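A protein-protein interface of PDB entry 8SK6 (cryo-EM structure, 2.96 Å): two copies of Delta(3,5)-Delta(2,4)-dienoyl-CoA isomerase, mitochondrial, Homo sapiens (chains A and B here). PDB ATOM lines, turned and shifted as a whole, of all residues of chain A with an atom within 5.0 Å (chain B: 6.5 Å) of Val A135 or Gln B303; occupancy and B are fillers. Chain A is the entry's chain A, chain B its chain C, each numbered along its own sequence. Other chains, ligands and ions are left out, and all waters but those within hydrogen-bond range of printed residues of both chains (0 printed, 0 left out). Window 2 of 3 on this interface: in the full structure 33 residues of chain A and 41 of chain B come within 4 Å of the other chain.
The side-chain hydroxyl (OG) of Ser A139 sits at hydrogen-bond distance from the side-chain amide oxygen (OE1) of Gln B303 (3.3 Å).
OE1 of Gln B303 sits close to O of Met B299 (3.0 Å). The backbone carbonyl oxygen (O) of Val A135 lies within hydrogen-bond range of the side-chain hydroxyl (OG) of Ser A139, at 3.0 Å.
Among the printed residues, merely in contact across the chains: Val A135 with Gln B303 (3.4 Å), Ile A138 with Gln B303 (3.3 Å), Ser A139 with Met B299 (3.5 Å), Leu A142 with Met B299 (3.6 Å), Leu A142 with Leu B302 (3.9 Å) and Leu A142 with Gln B303 (3.7 Å).
Val A135 touches just one residue of chain B: Gln B303. Of the printed residues of chain B, Leu A142 touches Met B299 (3.6 Å), Leu B302 (3.9 Å) and Gln B303 (3.7 Å). Of the printed residues of chain A, Leu B302 touches Leu A142 (3.9 Å). Of the printed residues of chain B, Ile A138 touches Gln B303 (3.3 Å). Printed residues of chain A within 4 Å of Met B299: Ser A139 and Leu A142. Leu B307 touches none of the printed residues of chain A. Arg A137 touches none of the printed residues of chain B. The nearest residue of chain B that does not touch Val A135 is Met B299 (5.8 Å).
Of the 8 printed residues of chain A, 4 touch a printed residue of chain B. Printed residues of chain A that touch a printed residue of chain B: Val A135, Ile A138, Ser A139 and Leu A142. Of the 9 printed residues of chain B, 3 touch a printed residue of chain A. Printed residues of chain B that touch a printed residue of chain A: Met B299, Leu B302 and Gln B303. Hydrophobic or aromatic side chains of chain B that line the printed part of chain A: Met B299 and Leu B302. Among the printed residues, 7 pairs touch across the chains.
No position is printed for both chains. Of the 7 pairs that touch across the chains among the printed residues, none has its exchanged pair printed and touching as well.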
ATOM      1  N   ASP A 133     -17.560  13.761  10.840  1.00  0.00           N
ATOM      2  CA  ASP A 133     -17.693  12.720  11.854  1.00  0.00           C
ATOM      3  C   ASP A 133     -16.354  12.402  12.508  1.00  0.00           C
ATOM      4  O   ASP A 133     -16.279  12.223  13.730  1.00  0.00           O
ATOM      5  CB  ASP A 133     -18.299  11.462  11.233  1.00  0.00           C
ATOM      6  CG  ASP A 133     -19.601  11.740  10.513  1.00  0.00           C
ATOM      7  OD1 ASP A 133     -19.898  12.926  10.255  1.00  0.00           O
ATOM      8  OD2 ASP A 133     -20.334  10.776  10.209  1.00  0.00           O
ATOM      9  N   ASP A 134     -15.288  12.328  11.717  1.00  0.00           N
ATOM     10  CA  ASP A 134     -13.966  11.996  12.230  1.00  0.00           C
ATOM     11  C   ASP A 134     -12.955  12.953  11.608  1.00  0.00           C
ATOM     12  O   ASP A 134     -13.320  13.939  10.960  1.00  0.00           O
ATOM     13  CB  ASP A 134     -13.630  10.525  11.953  1.00  0.00           C
ATOM     14  CG  ASP A 134     -13.877  10.137  10.515  1.00  0.00           C
ATOM     15  OD1 ASP A 134     -14.393  10.984   9.760  1.00  0.00           O
ATOM     16  OD2 ASP A 134     -13.561   8.989  10.140  1.00  0.00           O
ATOM     17  N   VAL A 135     -11.670  12.654  11.806  1.00  0.00           N
ATOM     18  CA  VAL A 135     -10.613  13.568  11.389  1.00  0.00           C
ATOM     19  C   VAL A 135     -10.568  13.696   9.872  1.00  0.00           C
ATOM     20  O   VAL A 135     -10.362  14.791   9.335  1.00  0.00           O
ATOM     21  CB  VAL A 135      -9.261  13.110  11.961  1.00  0.00           C
ATOM     22  CG1 VAL A 135      -8.148  14.034  11.503  1.00  0.00           C
ATOM     23  CG2 VAL A 135      -9.323  13.057  13.476  1.00  0.00           C
ATOM     24  N   ALA A 136     -10.755  12.587   9.155  1.00  0.00           N
ATOM     25  CA  ALA A 136     -10.661  12.618   7.698  1.00  0.00           C
ATOM     26  C   ALA A 136     -11.731  13.522   7.095  1.00  0.00           C
ATOM     27  O   ALA A 136     -11.458  14.300   6.175  1.00  0.00           O
ATOM     28  CB  ALA A 136     -10.771  11.200   7.137  1.00  0.00           C
ATOM     29  N   ARG A 137     -12.962  13.426   7.600  1.00  0.00           N
ATOM     30  CA  ARG A 137     -14.023  14.306   7.122  1.00  0.00           C
ATOM     31  C   ARG A 137     -13.733  15.758   7.478  1.00  0.00           C
ATOM     32  O   ARG A 137     -14.006  16.667   6.685  1.00  0.00           O
ATOM     33  CB  ARG A 137     -15.373  13.871   7.695  1.00  0.00           C
ATOM     34  CG  ARG A 137     -16.119  12.835   6.865  1.00  0.00           C
ATOM     35  CD  ARG A 137     -15.425  11.488   6.888  1.00  0.00           C
ATOM     36  NE  ARG A 137     -16.196  10.457   6.204  1.00  0.00           N
ATOM     37  CZ  ARG A 137     -15.858   9.175   6.167  1.00  0.00           C
ATOM     38  NH1 ARG A 137     -14.772   8.729   6.774  1.00  0.00           N
ATOM     39  NH2 ARG A 137     -16.632   8.320   5.505  1.00  0.00           N
ATOM     40  N   ILE A 138     -13.186  15.995   8.672  1.00  0.00           N
ATOM     41  CA  ILE A 138     -12.850  17.355   9.085  1.00  0.00           C
ATOM     42  C   ILE A 138     -11.760  17.932   8.191  1.00  0.00           C
ATOM     43  O   ILE A 138     -11.805  19.110   7.814  1.00  0.00           O
ATOM     44  CB  ILE A 138     -12.436  17.374  10.568  1.00  0.00           C
ATOM     45  CG1 ILE A 138     -13.636  17.055  11.459  1.00  0.00           C
ATOM     46  CG2 ILE A 138     -11.845  18.719  10.942  1.00  0.00           C
ATOM     47  CD1 ILE A 138     -13.302  17.010  12.929  1.00  0.00           C
ATOM     48  N   SER A 139     -10.766  17.115   7.838  1.00  0.00           N
ATOM     49  CA  SER A 139      -9.670  17.596   7.001  1.00  0.00           C
ATOM     50  C   SER A 139     -10.179  18.056   5.640  1.00  0.00           C
ATOM     51  O   SER A 139      -9.741  19.087   5.119  1.00  0.00           O
ATOM     52  CB  SER A 139      -8.614  16.503   6.843  1.00  0.00           C
ATOM     53  OG  SER A 139      -8.056  16.152   8.096  1.00  0.00           O
ATOM     54  N   LEU A 142     -11.858  21.377   6.278  1.00  0.00           N
ATOM     55  CA  LEU A 142     -10.917  22.467   6.518  1.00  0.00           C
ATOM     56  C   LEU A 142     -10.180  22.855   5.243  1.00  0.00           C
ATOM     57  O   LEU A 142      -9.949  24.042   4.985  1.00  0.00           O
ATOM     58  CB  LEU A 142      -9.930  22.081   7.616  1.00  0.00           C
ATOM     59  CG  LEU A 142     -10.510  21.978   9.025  1.00  0.00           C
ATOM     60  CD1 LEU A 142      -9.417  21.669  10.030  1.00  0.00           C
ATOM     61  CD2 LEU A 142     -11.236  23.259   9.395  1.00  0.00           C
ATOM     62  N   ASN B 298      -2.007  22.115   6.356  1.00  0.00           N
ATOM     63  CA  ASN B 298      -2.695  22.722   7.488  1.00  0.00           C
ATOM     64  C   ASN B 298      -4.043  22.083   7.793  1.00  0.00           C
ATOM     65  O   ASN B 298      -4.582  22.316   8.877  1.00  0.00           O
ATOM     66  CB  ASN B 298      -2.891  24.220   7.251  1.00  0.00           C
ATOM     67  CG  ASN B 298      -1.806  25.056   7.894  1.00  0.00           C
ATOM     68  OD1 ASN B 298      -0.674  24.604   8.055  1.00  0.00           O
ATOM     69  ND2 ASN B 298      -2.149  26.278   8.274  1.00  0.00           N
ATOM     70  N   MET B 299      -4.600  21.289   6.877  1.00  0.00           N
ATOM     71  CA  MET B 299      -5.895  20.676   7.148  1.00  0.00           C
ATOM     72  C   MET B 299      -5.832  19.702   8.316  1.00  0.00           C
ATOM     73  O   MET B 299      -6.873  19.381   8.899  1.00  0.00           O
ATOM     74  CB  MET B 299      -6.424  19.967   5.901  1.00  0.00           C
ATOM     75  CG  MET B 299      -5.596  18.785   5.447  1.00  0.00           C
ATOM     76  SD  MET B 299      -6.245  18.039   3.942  1.00  0.00           S
ATOM     77  CE  MET B 299      -5.001  16.793   3.626  1.00  0.00           C
ATOM     78  N   SER B 300      -4.639  19.228   8.672  1.00  0.00           N
ATOM     79  CA  SER B 300      -4.436  18.411   9.861  1.00  0.00           C
ATOM     80  C   SER B 300      -3.878  19.205  11.032  1.00  0.00           C
ATOM     81  O   SER B 300      -4.293  18.990  12.174  1.00  0.00           O
ATOM     82  CB  SER B 300      -3.493  17.247   9.549  1.00  0.00           C
ATOM     83  OG  SER B 300      -2.242  17.722   9.086  1.00  0.00           O
ATOM     84  N   MET B 301      -2.946  20.124  10.769  1.00  0.00           N
ATOM     85  CA  MET B 301      -2.311  20.878  11.843  1.00  0.00           C
ATOM     86  C   MET B 301      -3.247  21.897  12.476  1.00  0.00           C
ATOM     87  O   MET B 301      -2.956  22.385  13.571  1.00  0.00           O
ATOM     88  CB  MET B 301      -1.059  21.577  11.318  1.00  0.00           C
ATOM     89  CG  MET B 301      -0.068  20.642  10.651  1.00  0.00           C
ATOM     90  SD  MET B 301       0.439  19.296  11.732  1.00  0.00           S
ATOM     91  CE  MET B 301       1.458  18.339  10.616  1.00  0.00           C
ATOM     92  N   LEU B 302      -4.356  22.237  11.817  1.00  0.00           N
ATOM     93  CA  LEU B 302      -5.323  23.142  12.426  1.00  0.00           C
ATOM     94  C   LEU B 302      -6.088  22.485  13.564  1.00  0.00           C
ATOM     95  O   LEU B 302      -6.545  23.185  14.473  1.00  0.00           O
ATOM     96  CB  LEU B 302      -6.307  23.659  11.376  1.00  0.00           C
ATOM     97  CG  LEU B 302      -5.799  24.781  10.472  1.00  0.00           C
ATOM     98  CD1 LEU B 302      -6.890  25.243   9.522  1.00  0.00           C
ATOM     99  CD2 LEU B 302      -5.294  25.939  11.308  1.00  0.00           C
ATOM    100  N   GLN B 303      -6.235  21.161  13.537  1.00  0.00           N
ATOM    101  CA  GLN B 303      -6.958  20.434  14.578  1.00  0.00           C
ATOM    102  C   GLN B 303      -5.999  20.126  15.727  1.00  0.00           C
ATOM    103  O   GLN B 303      -5.574  18.990  15.950  1.00  0.00           O
ATOM    104  CB  GLN B 303      -7.573  19.166  14.007  1.00  0.00           C
ATOM    105  CG  GLN B 303      -8.177  19.343  12.629  1.00  0.00           C
ATOM    106  CD  GLN B 303      -8.601  18.031  12.013  1.00  0.00           C
ATOM    107  OE1 GLN B 303      -8.666  17.897  10.793  1.00  0.00           O
ATOM    108  NE2 GLN B 303      -8.895  17.051  12.858  1.00  0.00           N
ATOM    109  N   THR B 304      -5.655  21.173  16.468  1.00  0.00           N
ATOM    110  CA  THR B 304      -4.709  21.061  17.567  1.00  0.00           C
ATOM    111  C   THR B 304      -5.232  21.802  18.787  1.00  0.00           C
ATOM    112  O   THR B 304      -6.022  22.743  18.674  1.00  0.00           O
ATOM    113  CB  THR B 304      -3.331  21.614  17.183  1.00  0.00           C
ATOM    114  OG1 THR B 304      -2.445  21.505  18.304  1.00  0.00           O
ATOM    115  CG2 THR B 304      -3.437  23.073  16.768  1.00  0.00           C
ATOM    116  N   GLN B 305      -4.785  21.358  19.964  1.00  0.00           N
ATOM    117  CA  GLN B 305      -5.113  22.061  21.196  1.00  0.00           C
ATOM    118  C   GLN B 305      -4.338  23.362  21.336  1.00  0.00           C
ATOM    119  O   GLN B 305      -4.743  24.230  22.115  1.00  0.00           O
ATOM    120  CB  GLN B 305      -4.843  21.165  22.405  1.00  0.00           C
ATOM    121  CG  GLN B 305      -5.558  19.828  22.360  1.00  0.00           C
ATOM    122  CD  GLN B 305      -7.066  19.973  22.337  1.00  0.00           C
ATOM    123  OE1 GLN B 305      -7.619  20.926  22.886  1.00  0.00           O
ATOM    124  NE2 GLN B 305      -7.741  19.026  21.696  1.00  0.00           N
ATOM    125  N   LEU B 307      -4.088  25.685  19.096  1.00  0.00           N
ATOM    126  CA  LEU B 307      -4.917  26.748  18.539  1.00  0.00           C
ATOM    127  C   LEU B 307      -5.931  27.240  19.563  1.00  0.00           C
ATOM    128  O   LEU B 307      -6.186  28.444  19.671  1.00  0.00           O
ATOM    129  CB  LEU B 307      -5.615  26.250  17.272  1.00  0.00           C
ATOM    130  CG  LEU B 307      -6.110  27.281  16.255  1.00  0.00           C
ATOM    131  CD1 LEU B 307      -6.222  26.635  14.886  1.00  0.00           C
ATOM    132  CD2 LEU B 307      -7.449  27.875  16.663  1.00  0.00           C
